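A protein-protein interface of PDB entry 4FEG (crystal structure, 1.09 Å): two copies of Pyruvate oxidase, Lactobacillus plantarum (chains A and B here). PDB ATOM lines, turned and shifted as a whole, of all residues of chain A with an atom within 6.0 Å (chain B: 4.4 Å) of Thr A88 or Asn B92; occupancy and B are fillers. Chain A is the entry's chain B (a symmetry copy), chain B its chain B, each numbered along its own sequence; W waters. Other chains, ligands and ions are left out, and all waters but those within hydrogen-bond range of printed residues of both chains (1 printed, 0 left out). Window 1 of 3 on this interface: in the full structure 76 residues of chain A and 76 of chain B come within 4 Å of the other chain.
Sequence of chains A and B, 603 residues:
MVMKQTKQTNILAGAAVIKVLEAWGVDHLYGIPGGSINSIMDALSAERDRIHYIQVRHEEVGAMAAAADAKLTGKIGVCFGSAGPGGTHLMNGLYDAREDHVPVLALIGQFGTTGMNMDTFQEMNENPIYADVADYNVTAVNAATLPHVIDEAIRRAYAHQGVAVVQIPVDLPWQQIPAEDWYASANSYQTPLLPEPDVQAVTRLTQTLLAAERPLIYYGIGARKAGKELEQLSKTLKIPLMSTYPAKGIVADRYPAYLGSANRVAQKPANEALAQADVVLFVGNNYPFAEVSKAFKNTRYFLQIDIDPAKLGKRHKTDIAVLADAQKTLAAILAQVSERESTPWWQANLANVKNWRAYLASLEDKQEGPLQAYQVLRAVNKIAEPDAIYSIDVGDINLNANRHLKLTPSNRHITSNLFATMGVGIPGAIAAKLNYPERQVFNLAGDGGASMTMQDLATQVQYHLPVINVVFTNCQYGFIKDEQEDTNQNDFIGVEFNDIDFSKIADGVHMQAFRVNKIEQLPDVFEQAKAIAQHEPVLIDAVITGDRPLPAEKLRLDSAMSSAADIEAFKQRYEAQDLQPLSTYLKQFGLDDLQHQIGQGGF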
ATOM      1  N   SER A  82      20.572  16.504  -0.367  1.00  0.00           N
ATOM      2  CA  SER A  82      21.553  16.868  -1.378  1.00  0.00           C
ATOM      3  C   SER A  82      22.970  16.727  -0.834  1.00  0.00           C
ATOM      4  O   SER A  82      23.216  16.628   0.365  1.00  0.00           O
ATOM      5  CB  SER A  82      21.241  18.275  -1.841  1.00  0.00           C
ATOM      6  OG  SER A  82      21.356  19.220  -0.776  1.00  0.00           O
ATOM      7  N   GLY A  84      26.654  17.034   0.534  1.00  0.00           N
ATOM      8  CA  GLY A  84      27.206  17.860   1.597  1.00  0.00           C
ATOM      9  C   GLY A  84      26.137  18.223   2.600  1.00  0.00           C
ATOM     10  O   GLY A  84      25.641  17.355   3.317  1.00  0.00           O
ATOM     11  N   PRO A  85      25.773  19.501   2.683  1.00  0.00           N
ATOM     12  CA  PRO A  85      24.904  19.964   3.770  1.00  0.00           C
ATOM     13  C   PRO A  85      23.484  19.447   3.761  1.00  0.00           C
ATOM     14  O   PRO A  85      22.821  19.455   4.811  1.00  0.00           O
ATOM     15  CB  PRO A  85      24.903  21.487   3.547  1.00  0.00           C
ATOM     16  CG  PRO A  85      25.250  21.677   2.094  1.00  0.00           C
ATOM     17  CD  PRO A  85      26.291  20.616   1.862  1.00  0.00           C
ATOM     18  N   GLY A  86      22.940  19.040   2.607  1.00  0.00           N
ATOM     19  CA  GLY A  86      21.612  18.422   2.638  1.00  0.00           C
ATOM     20  C   GLY A  86      21.617  17.147   3.434  1.00  0.00           C
ATOM     21  O   GLY A  86      20.799  16.943   4.340  1.00  0.00           O
ATOM     22  N   GLY A  87      22.569  16.266   3.108  1.00  0.00           N
ATOM     23  CA  GLY A  87      22.712  15.016   3.807  1.00  0.00           C
ATOM     24  C   GLY A  87      23.104  15.166   5.277  1.00  0.00           C
ATOM     25  O   GLY A  87      22.556  14.465   6.135  1.00  0.00           O
ATOM     26  N   THR A  88      24.035  16.062   5.595  1.00  0.00           N
ATOM     27  CA  THR A  88      24.421  16.160   6.978  1.00  0.00           C
ATOM     28  C   THR A  88      23.281  16.694   7.863  1.00  0.00           C
ATOM     29  O   THR A  88      23.211  16.366   9.040  1.00  0.00           O
ATOM     30  CB  THR A  88      25.691  17.010   7.181  1.00  0.00           C
ATOM     31  OG1 THR A  88      25.567  18.288   6.582  1.00  0.00           O
ATOM     32  CG2 THR A  88      26.929  16.322   6.562  1.00  0.00           C
ATOM     33  N   HIS A  89      22.368  17.452   7.248  1.00  0.00           N
ATOM     34  CA  HIS A  89      21.196  17.860   7.986  1.00  0.00           C
ATOM     35  C   HIS A  89      20.300  16.678   8.362  1.00  0.00           C
ATOM     36  O   HIS A  89      19.461  16.838   9.252  1.00  0.00           O
ATOM     37  CB  HIS A  89      20.375  18.863   7.186  1.00  0.00           C
ATOM     38  CG  HIS A  89      20.619  20.293   7.489  1.00  0.00           C
ATOM     39  ND1 HIS A  89      20.021  21.299   6.765  1.00  0.00           N
ATOM     40  CD2 HIS A  89      21.305  20.941   8.469  1.00  0.00           C
ATOM     41  CE1 HIS A  89      20.343  22.486   7.299  1.00  0.00           C
ATOM     42  NE2 HIS A  89      21.133  22.291   8.338  1.00  0.00           N
ATOM     43  N   LEU A  90      20.413  15.540   7.700  1.00  0.00           N
ATOM     44  CA  LEU A  90      19.571  14.392   8.043  1.00  0.00           C
ATOM     45  C   LEU A  90      19.938  13.806   9.394  1.00  0.00           C
ATOM     46  O   LEU A  90      19.159  12.989   9.936  1.00  0.00           O
ATOM     47  CB  LEU A  90      19.774  13.278   7.009  1.00  0.00           C
ATOM     48  CG  LEU A  90      19.401  13.616   5.578  1.00  0.00           C
ATOM     49  CD1 LEU A  90      19.850  12.506   4.668  1.00  0.00           C
ATOM     50  CD2 LEU A  90      17.928  13.856   5.376  1.00  0.00           C
ATOM     51  N   MET A  91      21.146  14.058   9.892  1.00  0.00           N
ATOM     52  CA  MET A  91      21.699  13.271  10.982  1.00  0.00           C
ATOM     53  C   MET A  91      20.805  13.084  12.173  1.00  0.00           C
ATOM     54  O   MET A  91      20.713  11.968  12.680  1.00  0.00           O
ATOM     55  CB  MET A  91      23.046  13.834  11.446  1.00  0.00           C
ATOM     56  CG  MET A  91      24.162  13.542  10.476  1.00  0.00           C
ATOM     57  SD  MET A  91      24.387  11.787  10.245  1.00  0.00           S
ATOM     58  CE  MET A  91      25.752  11.812   9.109  1.00  0.00           C
ATOM     59  N   ASN A  92      20.173  14.125  12.693  1.00  0.00           N
ATOM     60  CA  ASN A  92      19.410  13.894  13.944  1.00  0.00           C
ATOM     61  C   ASN A  92      18.292  12.889  13.734  1.00  0.00           C
ATOM     62  O   ASN A  92      17.937  12.139  14.641  1.00  0.00           O
ATOM     63  CB  ASN A  92      18.880  15.187  14.553  1.00  0.00           C
ATOM     64  CG  ASN A  92      19.987  15.847  15.324  1.00  0.00           C
ATOM     65  OD1 ASN A  92      21.102  16.012  14.828  1.00  0.00           O
ATOM     66  ND2 ASN A  92      19.706  16.241  16.532  1.00  0.00           N
ATOM     67  N   ILE A 129      30.935  10.028   6.253  1.00  0.00           N
ATOM     68  CA  ILE A 129      30.008  10.819   7.023  1.00  0.00           C
ATOM     69  C   ILE A 129      28.980   9.911   7.718  1.00  0.00           C
ATOM     70  O   ILE A 129      28.541  10.196   8.842  1.00  0.00           O
ATOM     71  CB  ILE A 129      29.320  11.866   6.128  1.00  0.00           C
ATOM     72  CG1 ILE A 129      30.343  12.801   5.448  1.00  0.00           C
ATOM     73  CG2 ILE A 129      28.268  12.636   6.901  1.00  0.00           C
ATOM     74  CD1 ILE A 129      29.740  13.774   4.490  1.00  0.00           C
ATOM     75  N   TYR A 130      28.572   8.852   7.013  1.00  0.00           N
ATOM     76  CA  TYR A 130      27.432   8.023   7.410  1.00  0.00           C
ATOM     77  C   TYR A 130      27.818   6.693   7.997  1.00  0.00           C
ATOM     78  O   TYR A 130      26.958   5.872   8.336  1.00  0.00           O
ATOM     79  CB  TYR A 130      26.449   7.821   6.183  1.00  0.00           C
ATOM     80  CG  TYR A 130      26.003   9.174   5.692  1.00  0.00           C
ATOM     81  CD1 TYR A 130      24.963   9.847   6.331  1.00  0.00           C
ATOM     82  CD2 TYR A 130      26.647   9.826   4.659  1.00  0.00           C
ATOM     83  CE1 TYR A 130      24.594  11.117   5.885  1.00  0.00           C
ATOM     84  CE2 TYR A 130      26.310  11.080   4.273  1.00  0.00           C
ATOM     85  CZ  TYR A 130      25.278  11.749   4.867  1.00  0.00           C
ATOM     86  OH  TYR A 130      24.895  13.024   4.562  1.00  0.00           O
ATOM     87  N   GLU B  60      23.184  23.981  15.413  1.00  0.00           N
ATOM     88  CA  GLU B  60      23.803  24.229  14.133  1.00  0.00           C
ATOM     89  C   GLU B  60      24.150  25.703  14.004  1.00  0.00           C
ATOM     90  O   GLU B  60      25.169  26.041  13.384  1.00  0.00           O
ATOM     91  CB  GLU B  60      23.002  23.794  12.891  1.00  0.00           C
ATOM     92  CG  GLU B  60      21.927  24.706  12.379  1.00  0.00           C
ATOM     93  CD  GLU B  60      21.248  24.097  11.175  1.00  0.00           C
ATOM     94  OE1 GLU B  60      21.970  23.944  10.133  1.00  0.00           O
ATOM     95  OE2 GLU B  60      20.061  23.739  11.275  1.00  0.00           O
ATOM     96  N   MET B  64      27.794  27.160  13.180  1.00  0.00           N
ATOM     97  CA  MET B  64      27.980  28.085  12.089  1.00  0.00           C
ATOM     98  C   MET B  64      28.538  29.400  12.564  1.00  0.00           C
ATOM     99  O   MET B  64      29.418  29.992  11.866  1.00  0.00           O
ATOM    100  CB  MET B  64      26.668  28.330  11.358  1.00  0.00           C
ATOM    101  CG  MET B  64      26.123  27.125  10.608  1.00  0.00           C
ATOM    102  SD  MET B  64      24.482  27.431   9.965  1.00  0.00           S
ATOM    103  CE  MET B  64      24.264  25.988   8.939  1.00  0.00           C
ATOM    104  N   LEU B  90      25.490  20.044  15.436  1.00  0.00           N
ATOM    105  CA  LEU B  90      26.589  20.941  15.071  1.00  0.00           C
ATOM    106  C   LEU B  90      27.060  20.707  13.648  1.00  0.00           C
ATOM    107  O   LEU B  90      27.812  21.549  13.108  1.00  0.00           O
ATOM    108  CB  LEU B  90      27.793  20.678  15.983  1.00  0.00           C
ATOM    109  CG  LEU B  90      27.575  20.918  17.466  1.00  0.00           C
ATOM    110  CD1 LEU B  90      28.768  20.420  18.234  1.00  0.00           C
ATOM    111  CD2 LEU B  90      27.328  22.362  17.816  1.00  0.00           C
ATOM    112  N   MET B  91      26.786  19.540  13.069  1.00  0.00           N
ATOM    113  CA  MET B  91      27.484  19.103  11.871  1.00  0.00           C
ATOM    114  C   MET B  91      27.550  20.100  10.752  1.00  0.00           C
ATOM    115  O   MET B  91      28.615  20.263  10.161  1.00  0.00           O
ATOM    116  CB  MET B  91      26.906  17.787  11.341  1.00  0.00           C
ATOM    117  CG  MET B  91      27.301  16.599  12.180  1.00  0.00           C
ATOM    118  SD  MET B  91      29.073  16.399  12.239  1.00  0.00           S
ATOM    119  CE  MET B  91      29.172  14.941  13.248  1.00  0.00           C
ATOM    120  N   ASN B  92      26.456  20.748  10.380  1.00  0.00           N
ATOM    121  CA  ASN B  92      26.563  21.622   9.186  1.00  0.00           C
ATOM    122  C   ASN B  92      27.563  22.742   9.406  1.00  0.00           C
ATOM    123  O   ASN B  92      28.224  23.192   8.473  1.00  0.00           O
ATOM    124  CB  ASN B  92      25.213  22.169   8.739  1.00  0.00           C
ATOM    125  CG  ASN B  92      24.507  21.116   7.933  1.00  0.00           C
ATOM    126  OD1 ASN B  92      24.406  19.959   8.342  1.00  0.00           O
ATOM    127  ND2 ASN B  92      24.003  21.490   6.794  1.00  0.00           N
ATOM    128  N   GLY B  93      27.682  23.256  10.653  1.00  0.00           N
ATOM    129  CA  GLY B  93      28.699  24.250  10.922  1.00  0.00           C
ATOM    130  C   GLY B  93      30.099  23.713  11.030  1.00  0.00           C
ATOM    131  O   GLY B  93      31.049  24.376  10.614  1.00  0.00           O
ATOM    132  N   LEU B  94      30.249  22.489  11.538  1.00  0.00           N
ATOM    133  CA  LEU B  94      31.587  21.882  11.606  1.00  0.00           C
ATOM    134  C   LEU B  94      32.131  21.581  10.207  1.00  0.00           C
ATOM    135  O   LEU B  94      33.292  21.808   9.919  1.00  0.00           O
ATOM    136  CB  LEU B  94      31.570  20.657  12.499  1.00  0.00           C
ATOM    137  CG  LEU B  94      31.139  20.882  13.950  1.00  0.00           C
ATOM    138  CD1 LEU B  94      31.252  19.582  14.730  1.00  0.00           C
ATOM    139  CD2 LEU B  94      31.853  22.009  14.636  1.00  0.00           C
ATOM    140  N   TYR B  95      31.247  21.055   9.325  1.00  0.00           N
ATOM    141  CA  TYR B  95      31.692  20.781   7.947  1.00  0.00           C
ATOM    142  C   TYR B  95      32.003  22.078   7.237  1.00  0.00           C
ATOM    143  O   TYR B  95      32.919  22.166   6.431  1.00  0.00           O
ATOM    144  CB  TYR B  95      30.630  19.953   7.159  1.00  0.00           C
ATOM    145  CG  TYR B  95      30.848  18.479   7.433  1.00  0.00           C
ATOM    146  CD1 TYR B  95      31.711  17.737   6.645  1.00  0.00           C
ATOM    147  CD2 TYR B  95      30.245  17.823   8.486  1.00  0.00           C
ATOM    148  CE1 TYR B  95      31.941  16.398   6.885  1.00  0.00           C
ATOM    149  CE2 TYR B  95      30.505  16.492   8.767  1.00  0.00           C
ATOM    150  CZ  TYR B  95      31.352  15.782   7.959  1.00  0.00           C
ATOM    151  OH  TYR B  95      31.650  14.464   8.276  1.00  0.00           O
ATOM    152  N   ASP B  96      31.246  23.164   7.533  1.00  0.00           N
ATOM    153  CA  ASP B  96      31.565  24.478   6.972  1.00  0.00           C
ATOM    154  C   ASP B  96      32.970  24.886   7.386  1.00  0.00           C
ATOM    155  O   ASP B  96      33.761  25.361   6.574  1.00  0.00           O
ATOM    156  CB  ASP B  96      30.521  25.494   7.426  1.00  0.00           C
ATOM    157  CG  ASP B  96      30.740  26.845   6.766  1.00  0.00           C
ATOM    158  OD1 ASP B  96      30.952  26.912   5.548  1.00  0.00           O
ATOM    159  OD2 ASP B  96      30.637  27.845   7.509  1.00  0.00           O
ATOM    160  N   PHE B 419      31.480  24.166   1.332  1.00  0.00           N
ATOM    161  CA  PHE B 419      30.406  23.286   1.769  1.00  0.00           C
ATOM    162  C   PHE B 419      29.049  23.803   1.329  1.00  0.00           C
ATOM    163  O   PHE B 419      28.123  23.058   1.084  1.00  0.00           O
ATOM    164  CB  PHE B 419      30.499  23.082   3.277  1.00  0.00           C
ATOM    165  CG  PHE B 419      29.654  21.971   3.848  1.00  0.00           C
ATOM    166  CD1 PHE B 419      29.884  20.645   3.440  1.00  0.00           C
ATOM    167  CD2 PHE B 419      28.680  22.207   4.807  1.00  0.00           C
ATOM    168  CE1 PHE B 419      29.133  19.614   4.001  1.00  0.00           C
ATOM    169  CE2 PHE B 419      27.926  21.160   5.365  1.00  0.00           C
ATOM    170  CZ  PHE B 419      28.166  19.873   4.944  1.00  0.00           C
ATOM    171  N   THR B 421      26.595  25.341   2.931  1.00  0.00           N
ATOM    172  CA  THR B 421      25.391  25.082   3.691  1.00  0.00           C
ATOM    173  C   THR B 421      24.488  26.305   3.737  1.00  0.00           C
ATOM    174  O   THR B 421      24.854  27.404   4.158  1.00  0.00           O
ATOM    175  CB  THR B 421      25.707  24.606   5.117  1.00  0.00           C
ATOM    176  OG1 THR B 421      24.453  24.304   5.776  1.00  0.00           O
ATOM    177  CG2 THR B 421      26.534  25.536   5.990  1.00  0.00           C
HETATM  178  O   HOH W   1      20.681  25.458   8.003  1.00  0.00           O
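A ring nitrogen (NE2) of His A89 lies within hydrogen-bond range of the side-chain carboxylate of Glu B60 (2.6 Å). O of Pro A85 sits at hydrogen-bond distance from ND2 of Asn B92 (3.1 Å). OD1 of Asn B92 is in hydrogen-bond range of OG1 of Thr A88 (2.7 Å). The side-chain amide nitrogen (ND2) of Asn B92 sits close to a ring nitrogen (NE2) of His A89, at 3.4 Å.
The side-chain hydroxyl of Thr B421 is in hydrogen-bond range of the side-chain amide nitrogen of Asn B92. O of Gly A84 lies within hydrogen-bond range of OG1 of Thr A88. The backbone carbonyl oxygen (O) of Pro A85 lies close to the side-chain hydroxyl (OG1) of Thr A88, at 3.5 Å. The backbone NH (N) of Thr A88 sits at hydrogen-bond distance from the side-chain hydroxyl (OH) of Tyr A130 (3.3 Å).
Phe B419 touches Gly A84. CD of Pro A85 touches O of Phe B419, 3.2 Å away. Pro A85 touches Thr B421 (CB to CB, 3.6 Å). Phe B419 touches Thr A88. Ile A129 touches Tyr B95 (CG1 to OH, 3.5 Å).
Thr A88 touches two residues of chain B. Printed residues of chain A within 4 Å of Glu B60: His A89. Asn B92 touches just these residues of chain A: Pro A85, Thr A88 and His A89. Of the printed residues of chain A, Tyr B95 touches Ile A129. Of the printed residues of chain A, Phe B419 touches Gly A84 (3.5 Å), Pro A85 (3.2 Å) and Thr A88 (3.5 Å). The nearest residue of chain B that does not touch Thr A88 is Tyr B95 (4.1 Å). The nearest printed residue of chain B that does not touch Ile A129 is Phe B419 (5.9 Å).
Of the 11 printed residues of chain B, 5 touch a printed residue of chain A. Printed residues of chain B that touch a printed residue of chain A: Glu B60, Asn B92, Tyr B95, Phe B419 and Thr B421. Hydrophobic or aromatic side chains of chain B that line the printed part of chain A: Tyr B95 and Phe B419. Among the printed residues, 9 pairs touch across the chains. Among the printed residues, no Asp or Glu carboxylate lies within 4 Å of a Lys or Arg side-chain nitrogen of the other chain.
Positions printed for both chains: 90, 91 and 92. Of the 9 pairs that touch across the chains among the printed residues, none has its exchanged pair printed and touching as well.
Water W1 lies within hydrogen-bond range of OE1 of Glu B60 (2.9 Å) and NE2 of His A89 (3.2 Å).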
